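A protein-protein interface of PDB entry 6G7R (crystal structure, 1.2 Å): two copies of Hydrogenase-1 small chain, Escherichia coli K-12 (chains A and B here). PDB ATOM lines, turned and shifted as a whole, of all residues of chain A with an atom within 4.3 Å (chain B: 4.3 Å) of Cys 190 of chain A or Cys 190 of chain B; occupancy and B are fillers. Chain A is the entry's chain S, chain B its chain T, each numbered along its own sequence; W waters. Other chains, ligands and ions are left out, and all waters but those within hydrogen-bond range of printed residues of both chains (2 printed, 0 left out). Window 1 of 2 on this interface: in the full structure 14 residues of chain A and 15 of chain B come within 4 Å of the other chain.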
ATOM      1  N   ILE A 186      14.616  -5.552 -25.307  1.00  0.00           N
ATOM      2  CA  ILE A 186      14.348  -6.817 -24.627  1.00  0.00           C
ATOM      3  C   ILE A 186      14.943  -7.979 -25.425  1.00  0.00           C
ATOM      4  O   ILE A 186      15.623  -8.869 -24.893  1.00  0.00           O
ATOM      5  CB  ILE A 186      12.824  -6.995 -24.400  1.00  0.00           C
ATOM      6  CG1 ILE A 186      12.235  -5.931 -23.454  1.00  0.00           C
ATOM      7  CG2 ILE A 186      12.470  -8.404 -23.991  1.00  0.00           C
ATOM      8  CD1 ILE A 186      12.785  -6.001 -22.058  1.00  0.00           C
ATOM      9  N   HIS A 187      14.643  -7.975 -26.715  1.00  0.00           N
ATOM     10  CA  HIS A 187      15.059  -9.038 -27.662  1.00  0.00           C
ATOM     11  C   HIS A 187      16.568  -9.049 -27.916  1.00  0.00           C
ATOM     12  O   HIS A 187      17.038 -10.060 -28.450  1.00  0.00           O
ATOM     13  CB  HIS A 187      14.247  -8.774 -28.941  1.00  0.00           C
ATOM     14  CG  HIS A 187      14.410  -9.674 -30.117  1.00  0.00           C
ATOM     15  ND1 HIS A 187      13.861 -10.939 -30.220  1.00  0.00           N
ATOM     16  CD2 HIS A 187      14.956  -9.419 -31.323  1.00  0.00           C
ATOM     17  CE1 HIS A 187      14.078 -11.423 -31.427  1.00  0.00           C
ATOM     18  NE2 HIS A 187      14.764 -10.510 -32.127  1.00  0.00           N
ATOM     19  N   ASP A 188      17.297  -7.995 -27.564  1.00  0.00           N
ATOM     20  CA  ASP A 188      18.749  -7.995 -27.673  1.00  0.00           C
ATOM     21  C   ASP A 188      19.426  -8.729 -26.505  1.00  0.00           C
ATOM     22  O   ASP A 188      20.638  -8.918 -26.573  1.00  0.00           O
ATOM     23  CB  ASP A 188      19.256  -6.537 -27.709  1.00  0.00           C
ATOM     24  CG  ASP A 188      18.859  -5.698 -28.901  1.00  0.00           C
ATOM     25  OD1 ASP A 188      18.542  -6.269 -29.971  1.00  0.00           O
ATOM     26  OD2 ASP A 188      18.754  -4.415 -28.711  1.00  0.00           O
ATOM     27  N   LYS A 189      18.681  -9.038 -25.440  1.00  0.00           N
ATOM     28  CA  LYS A 189      19.249  -9.699 -24.264  1.00  0.00           C
ATOM     29  C   LYS A 189      18.295 -10.799 -23.774  1.00  0.00           C
ATOM     30  O   LYS A 189      18.291 -11.139 -22.577  1.00  0.00           O
ATOM     31  CB  LYS A 189      19.549  -8.700 -23.146  1.00  0.00           C
ATOM     32  CG  LYS A 189      20.820  -7.900 -23.360  1.00  0.00           C
ATOM     33  CD  LYS A 189      22.073  -8.766 -23.366  1.00  0.00           C
ATOM     34  CE  LYS A 189      23.358  -8.085 -22.975  1.00  0.00           C
ATOM     35  NZ  LYS A 189      23.709  -7.027 -23.927  1.00  0.00           N
ATOM     36  N   CYS A 190      17.484 -11.360 -24.676  1.00  0.00           N
ATOM     37  CA  CYS A 190      16.490 -12.348 -24.258  1.00  0.00           C
ATOM     38  C   CYS A 190      17.068 -13.773 -24.318  1.00  0.00           C
ATOM     39  O   CYS A 190      17.666 -14.197 -25.339  1.00  0.00           O
ATOM     40  CB  CYS A 190      15.270 -12.287 -25.170  1.00  0.00           C
ATOM     41  SG  CYS A 190      13.972 -13.472 -24.675  1.00  0.00           S
ATOM     42  N   TYR A 191      16.907 -14.498 -23.215  1.00  0.00           N
ATOM     43  CA  TYR A 191      17.444 -15.863 -23.093  1.00  0.00           C
ATOM     44  C   TYR A 191      16.743 -16.838 -24.029  1.00  0.00           C
ATOM     45  O   TYR A 191      17.203 -17.970 -24.156  1.00  0.00           O
ATOM     46  CB  TYR A 191      17.433 -16.335 -21.628  1.00  0.00           C
ATOM     47  CG  TYR A 191      16.114 -16.885 -21.128  1.00  0.00           C
ATOM     48  CD1 TYR A 191      14.905 -16.201 -21.228  1.00  0.00           C
ATOM     49  CD2 TYR A 191      16.069 -18.133 -20.540  1.00  0.00           C
ATOM     50  CE1 TYR A 191      13.709 -16.739 -20.781  1.00  0.00           C
ATOM     51  CE2 TYR A 191      14.886 -18.690 -20.098  1.00  0.00           C
ATOM     52  CZ  TYR A 191      13.700 -17.999 -20.236  1.00  0.00           C
ATOM     53  OH  TYR A 191      12.508 -18.556 -19.858  1.00  0.00           O
ATOM     54  N   ARG A 192      15.654 -16.455 -24.733  1.00  0.00           N
ATOM     55  CA  ARG A 192      15.030 -17.343 -25.718  1.00  0.00           C
ATOM     56  C   ARG A 192      15.498 -17.026 -27.139  1.00  0.00           C
ATOM     57  O   ARG A 192      14.985 -17.650 -28.091  1.00  0.00           O
ATOM     58  CB  ARG A 192      13.509 -17.327 -25.605  1.00  0.00           C
ATOM     59  CG  ARG A 192      13.025 -17.784 -24.236  1.00  0.00           C
ATOM     60  CD  ARG A 192      11.523 -17.948 -24.142  1.00  0.00           C
ATOM     61  NE  ARG A 192      11.138 -18.357 -22.799  1.00  0.00           N
ATOM     62  CZ  ARG A 192      10.018 -18.970 -22.465  1.00  0.00           C
ATOM     63  NH1 ARG A 192       9.103 -19.278 -23.377  1.00  0.00           N
ATOM     64  NH2 ARG A 192       9.793 -19.219 -21.186  1.00  0.00           N
ATOM     65  N   ARG A 193      16.496 -16.181 -27.311  1.00  0.00           N
ATOM     66  CA  ARG A 193      16.963 -15.846 -28.658  1.00  0.00           C
ATOM     67  C   ARG A 193      17.524 -17.058 -29.394  1.00  0.00           C
ATOM     68  O   ARG A 193      17.373 -17.088 -30.624  1.00  0.00           O
ATOM     69  CB  ARG A 193      18.000 -14.735 -28.632  1.00  0.00           C
ATOM     70  CG  ARG A 193      17.433 -13.325 -28.713  1.00  0.00           C
ATOM     71  CD  ARG A 193      16.786 -13.002 -30.050  1.00  0.00           C
ATOM     72  NE  ARG A 193      17.672 -12.968 -31.192  1.00  0.00           N
ATOM     73  CZ  ARG A 193      18.131 -11.868 -31.791  1.00  0.00           C
ATOM     74  NH1 ARG A 193      17.971 -10.682 -31.230  1.00  0.00           N
ATOM     75  NH2 ARG A 193      18.789 -11.999 -32.934  1.00  0.00           N
ATOM     76  N   SER A 231      14.888  -8.395 -19.551  1.00  0.00           N
ATOM     77  CA  SER A 231      15.509  -9.661 -19.874  1.00  0.00           C
ATOM     78  C   SER A 231      16.902  -9.844 -19.246  1.00  0.00           C
ATOM     79  O   SER A 231      17.426 -10.946 -19.321  1.00  0.00           O
ATOM     80  CB  SER A 231      15.525  -9.840 -21.383  1.00  0.00           C
ATOM     81  OG  SER A 231      16.043  -8.691 -22.057  1.00  0.00           O
ATOM     82  N   ILE A 243       8.450 -12.844 -20.319  1.00  0.00           N
ATOM     83  CA  ILE A 243       8.794 -13.923 -21.234  1.00  0.00           C
ATOM     84  C   ILE A 243       9.221 -15.182 -20.470  1.00  0.00           C
ATOM     85  O   ILE A 243       8.853 -16.296 -20.873  1.00  0.00           O
ATOM     86  CB  ILE A 243       9.864 -13.418 -22.212  1.00  0.00           C
ATOM     87  CG1 ILE A 243       9.257 -12.434 -23.215  1.00  0.00           C
ATOM     88  CG2 ILE A 243      10.604 -14.555 -22.893  1.00  0.00           C
ATOM     89  CD1 ILE A 243      10.234 -11.364 -23.665  1.00  0.00           C
ATOM     90  N   ILE B 186      23.844 -24.537 -22.293  1.00  0.00           N
ATOM     91  CA  ILE B 186      23.963 -23.150 -21.828  1.00  0.00           C
ATOM     92  C   ILE B 186      23.590 -22.185 -22.971  1.00  0.00           C
ATOM     93  O   ILE B 186      22.834 -21.212 -22.794  1.00  0.00           O
ATOM     94  CB  ILE B 186      25.388 -22.888 -21.288  1.00  0.00           C
ATOM     95  CG1 ILE B 186      25.685 -23.728 -20.036  1.00  0.00           C
ATOM     96  CG2 ILE B 186      25.680 -21.425 -21.039  1.00  0.00           C
ATOM     97  CD1 ILE B 186      24.791 -23.390 -18.864  1.00  0.00           C
ATOM     98  N   HIS B 187      24.178 -22.444 -24.145  1.00  0.00           N
ATOM     99  CA  HIS B 187      24.055 -21.597 -25.326  1.00  0.00           C
ATOM    100  C   HIS B 187      22.647 -21.645 -25.939  1.00  0.00           C
ATOM    101  O   HIS B 187      22.322 -20.771 -26.736  1.00  0.00           O
ATOM    102  CB  HIS B 187      25.135 -22.053 -26.303  1.00  0.00           C
ATOM    103  CG  HIS B 187      25.239 -21.407 -27.629  1.00  0.00           C
ATOM    104  ND1 HIS B 187      25.853 -20.187 -27.825  1.00  0.00           N
ATOM    105  CD2 HIS B 187      24.975 -21.919 -28.855  1.00  0.00           C
ATOM    106  CE1 HIS B 187      25.928 -19.960 -29.118  1.00  0.00           C
ATOM    107  NE2 HIS B 187      25.393 -21.001 -29.789  1.00  0.00           N
ATOM    108  N   ASP B 188      21.816 -22.635 -25.558  1.00  0.00           N
ATOM    109  CA  ASP B 188      20.429 -22.710 -26.011  1.00  0.00           C
ATOM    110  C   ASP B 188      19.501 -21.782 -25.202  1.00  0.00           C
ATOM    111  O   ASP B 188      18.344 -21.609 -25.608  1.00  0.00           O
ATOM    112  CB  ASP B 188      19.925 -24.151 -25.870  1.00  0.00           C
ATOM    113  CG  ASP B 188      20.613 -25.208 -26.713  1.00  0.00           C
ATOM    114  OD1 ASP B 188      21.108 -24.877 -27.771  1.00  0.00           O
ATOM    115  OD2 ASP B 188      20.620 -26.413 -26.287  1.00  0.00           O
ATOM    116  N   LYS B 189      19.984 -21.233 -24.095  1.00  0.00           N
ATOM    117  CA  LYS B 189      19.168 -20.376 -23.201  1.00  0.00           C
ATOM    118  C   LYS B 189      20.010 -19.188 -22.730  1.00  0.00           C
ATOM    119  O   LYS B 189      19.748 -18.612 -21.677  1.00  0.00           O
ATOM    120  CB  LYS B 189      18.621 -21.189 -22.021  1.00  0.00           C
ATOM    121  CG  LYS B 189      17.389 -22.004 -22.367  1.00  0.00           C
ATOM    122  CD  LYS B 189      16.209 -21.154 -22.846  1.00  0.00           C
ATOM    123  CE  LYS B 189      14.853 -21.807 -22.642  1.00  0.00           C
ATOM    124  NZ  LYS B 189      14.720 -23.060 -23.414  1.00  0.00           N
ATOM    125  N   CYS B 190      21.033 -18.779 -23.511  1.00  0.00           N
ATOM    126  CA  CYS B 190      21.928 -17.705 -23.098  1.00  0.00           C
ATOM    127  C   CYS B 190      21.385 -16.352 -23.546  1.00  0.00           C
ATOM    128  O   CYS B 190      21.088 -16.145 -24.730  1.00  0.00           O
ATOM    129  CB  CYS B 190      23.337 -17.932 -23.632  1.00  0.00           C
ATOM    130  SG  CYS B 190      24.484 -16.620 -23.091  1.00  0.00           S
ATOM    131  N   TYR B 191      21.307 -15.420 -22.608  1.00  0.00           N
ATOM    132  CA  TYR B 191      20.807 -14.076 -22.895  1.00  0.00           C
ATOM    133  C   TYR B 191      21.728 -13.286 -23.809  1.00  0.00           C
ATOM    134  O   TYR B 191      21.331 -12.192 -24.240  1.00  0.00           O
ATOM    135  CB  TYR B 191      20.478 -13.314 -21.610  1.00  0.00           C
ATOM    136  CG  TYR B 191      21.636 -12.652 -20.932  1.00  0.00           C
ATOM    137  CD1 TYR B 191      22.814 -13.316 -20.608  1.00  0.00           C
ATOM    138  CD2 TYR B 191      21.561 -11.323 -20.590  1.00  0.00           C
ATOM    139  CE1 TYR B 191      23.861 -12.671 -19.974  1.00  0.00           C
ATOM    140  CE2 TYR B 191      22.613 -10.666 -19.980  1.00  0.00           C
ATOM    141  CZ  TYR B 191      23.787 -11.328 -19.689  1.00  0.00           C
ATOM    142  OH  TYR B 191      24.863 -10.667 -19.164  1.00  0.00           O
ATOM    143  N   ARG B 192      22.954 -13.748 -24.109  1.00  0.00           N
ATOM    144  CA  ARG B 192      23.796 -13.056 -25.083  1.00  0.00           C
ATOM    145  C   ARG B 192      23.702 -13.666 -26.480  1.00  0.00           C
ATOM    146  O   ARG B 192      24.446 -13.231 -27.384  1.00  0.00           O
ATOM    147  CB  ARG B 192      25.252 -12.990 -24.630  1.00  0.00           C
ATOM    148  CG  ARG B 192      25.394 -12.292 -23.290  1.00  0.00           C
ATOM    149  CD  ARG B 192      26.826 -12.083 -22.862  1.00  0.00           C
ATOM    150  NE  ARG B 192      26.890 -11.395 -21.583  1.00  0.00           N
ATOM    151  CZ  ARG B 192      27.921 -10.717 -21.095  1.00  0.00           C
ATOM    152  NH1 ARG B 192      29.032 -10.553 -21.810  1.00  0.00           N
ATOM    153  NH2 ARG B 192      27.815 -10.199 -19.866  1.00  0.00           N
ATOM    154  N   ARG B 193      22.732 -14.538 -26.709  1.00  0.00           N
ATOM    155  CA  ARG B 193      22.586 -15.161 -28.029  1.00  0.00           C
ATOM    156  C   ARG B 193      22.261 -14.130 -29.117  1.00  0.00           C
ATOM    157  O   ARG B 193      22.663 -14.339 -30.267  1.00  0.00           O
ATOM    158  CB  ARG B 193      21.512 -16.253 -28.034  1.00  0.00           C
ATOM    159  CG  ARG B 193      22.040 -17.677 -27.952  1.00  0.00           C
ATOM    160  CD  ARG B 193      23.072 -18.071 -29.010  1.00  0.00           C
ATOM    161  NE  ARG B 193      22.548 -18.577 -30.270  1.00  0.00           N
ATOM    162  CZ  ARG B 193      22.076 -19.810 -30.470  1.00  0.00           C
ATOM    163  NH1 ARG B 193      22.040 -20.687 -29.481  1.00  0.00           N
ATOM    164  NH2 ARG B 193      21.621 -20.145 -31.666  1.00  0.00           N
ATOM    165  N   SER B 231      22.236 -20.634 -17.467  1.00  0.00           N
ATOM    166  CA  SER B 231      21.747 -19.452 -18.186  1.00  0.00           C
ATOM    167  C   SER B 231      20.247 -19.234 -17.938  1.00  0.00           C
ATOM    168  O   SER B 231      19.776 -18.178 -18.331  1.00  0.00           O
ATOM    169  CB  SER B 231      22.063 -19.577 -19.655  1.00  0.00           C
ATOM    170  OG  SER B 231      21.726 -20.877 -20.155  1.00  0.00           O
ATOM    171  N   ILE B 243      28.790 -16.262 -17.507  1.00  0.00           N
ATOM    172  CA  ILE B 243      28.684 -15.382 -18.666  1.00  0.00           C
ATOM    173  C   ILE B 243      28.134 -14.008 -18.294  1.00  0.00           C
ATOM    174  O   ILE B 243      28.583 -12.994 -18.803  1.00  0.00           O
ATOM    175  CB  ILE B 243      27.867 -16.086 -19.748  1.00  0.00           C
ATOM    176  CG1 ILE B 243      28.669 -17.216 -20.388  1.00  0.00           C
ATOM    177  CG2 ILE B 243      27.354 -15.118 -20.799  1.00  0.00           C
ATOM    178  CD1 ILE B 243      27.839 -18.383 -20.822  1.00  0.00           C
HETATM  179  O   HOH W   1      19.824 -12.732 -26.521  1.00  0.00           O
HETATM  180  O   HOH W   2      19.204 -17.849 -26.073  1.00  0.00           O
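The backbone carbonyl oxygen (O) of His 187 of chain A sits at hydrogen-bond distance from the guanidinium group (NH1) of Arg 193 of chain A. O of Lys 189 of chain A sits close to OG of Ser 231 of chain A (3.4 Å). The guanidinium group (NH2) of Arg 192 of chain A lies within hydrogen-bond range of the side-chain hydroxyl (OH) of Tyr 191 of chain A, 3.1 Å away. OG of Ser 231 of chain B lies close to O of Lys 189 of chain B. The side-chain sulfur of Cys 190 of chain B sits close to the backbone NH of Arg 192 of chain B, 3.4 Å away. The side-chain hydroxyl (OH) of Tyr 191 of chain B lies within hydrogen-bond range of the guanidinium group (NH2) of Arg 192 of chain B.
Among the printed residues, merely in contact across the chains: Lys 189 of chain A with Tyr 191 of chain B (3.2 Å), Cys 190 of chain A with Cys 190 of chain B (3.98 Å), Cys 190 of chain A with Tyr 191 of chain B (3.96 Å), Tyr 191 of chain A with Lys 189 of chain B (3.2 Å), Tyr 191 of chain A with Cys 190 of chain B (3.97 Å), Tyr 191 of chain A with Tyr 191 of chain B (3.8 Å) and Arg 193 of chain A with Arg 193 of chain B (3.9 Å).
Printed residues of chain B within 4 Å of Lys 189 of chain A: Tyr 191. Printed residues of chain B within 4 Å of Cys 190 of chain A: Cys 190 (3.98 Å) and Tyr 191 (3.96 Å). Of the printed residues of chain B, Tyr 191 of chain A touches Lys 189 (3.2 Å), Cys 190 (3.97 Å) and Tyr 191 (3.8 Å). Of the printed residues of chain B, Arg 193 of chain A touches Arg 193. His 187 of chain B touches none of the printed residues of chain A. Asp 188 of chain B touches none of the printed residues of chain A. Printed residues of chain A within 4 Å of Lys 189 of chain B: Tyr 191 (3.2 Å). Printed residues of chain A within 4 Å of Cys 190 of chain B: Cys 190 (3.98 Å) and Tyr 191 (3.97 Å). Of the printed residues of chain A, Tyr 191 of chain B touches Lys 189, Cys 190 and Tyr 191. The nearest printed residue of chain B that does not touch Cys 190 of chain A is Arg 193 of chain B (5.1 Å). The nearest printed residue of chain A that does not touch Cys 190 of chain B is Arg 193 of chain A (5.2 Å).
Printed residues of chain A that touch a printed residue of chain B: Lys 189, Cys 190, Tyr 191 and Arg 193. Hydrophobic or aromatic side chains of chain A within 4 Å of the printed part of chain B: Tyr 191. Among the printed residues, 7 pairs touch across the chains.
Lys 189 of chain A touches Tyr 191 of chain B, and with the chains exchanged Tyr 191 of chain A touches Lys 189 of chain B. Cys 190 of chain B touches its own counterpart, Cys 190 of chain A. Cys 190 of chain A touches Tyr 191 of chain B, and with the chains exchanged Tyr 191 of chain A touches Cys 190 of chain B. Tyr 191 of chain B touches its own counterpart, Tyr 191 of chain A. 10 positions are printed for both chains. Of the 7 pairs that touch across the chains among the printed residues, 7 have their exchanged pair printed and touching as well.
Water W2 lies within hydrogen-bond range of the backbone carbonyl oxygen of Tyr 191 of chain A (2.8 Å), the backbone carbonyl oxygen of Cys 190 of chain B (2.9 Å) and the backbone NH of Arg 193 of chain A (3.4 Å). Water W1 lies within hydrogen-bond range of O of Tyr 191 of chain B (2.8 Å), O of Cys 190 of chain A (2.9 Å) and N of Arg 193 of chain B (3.4 Å).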
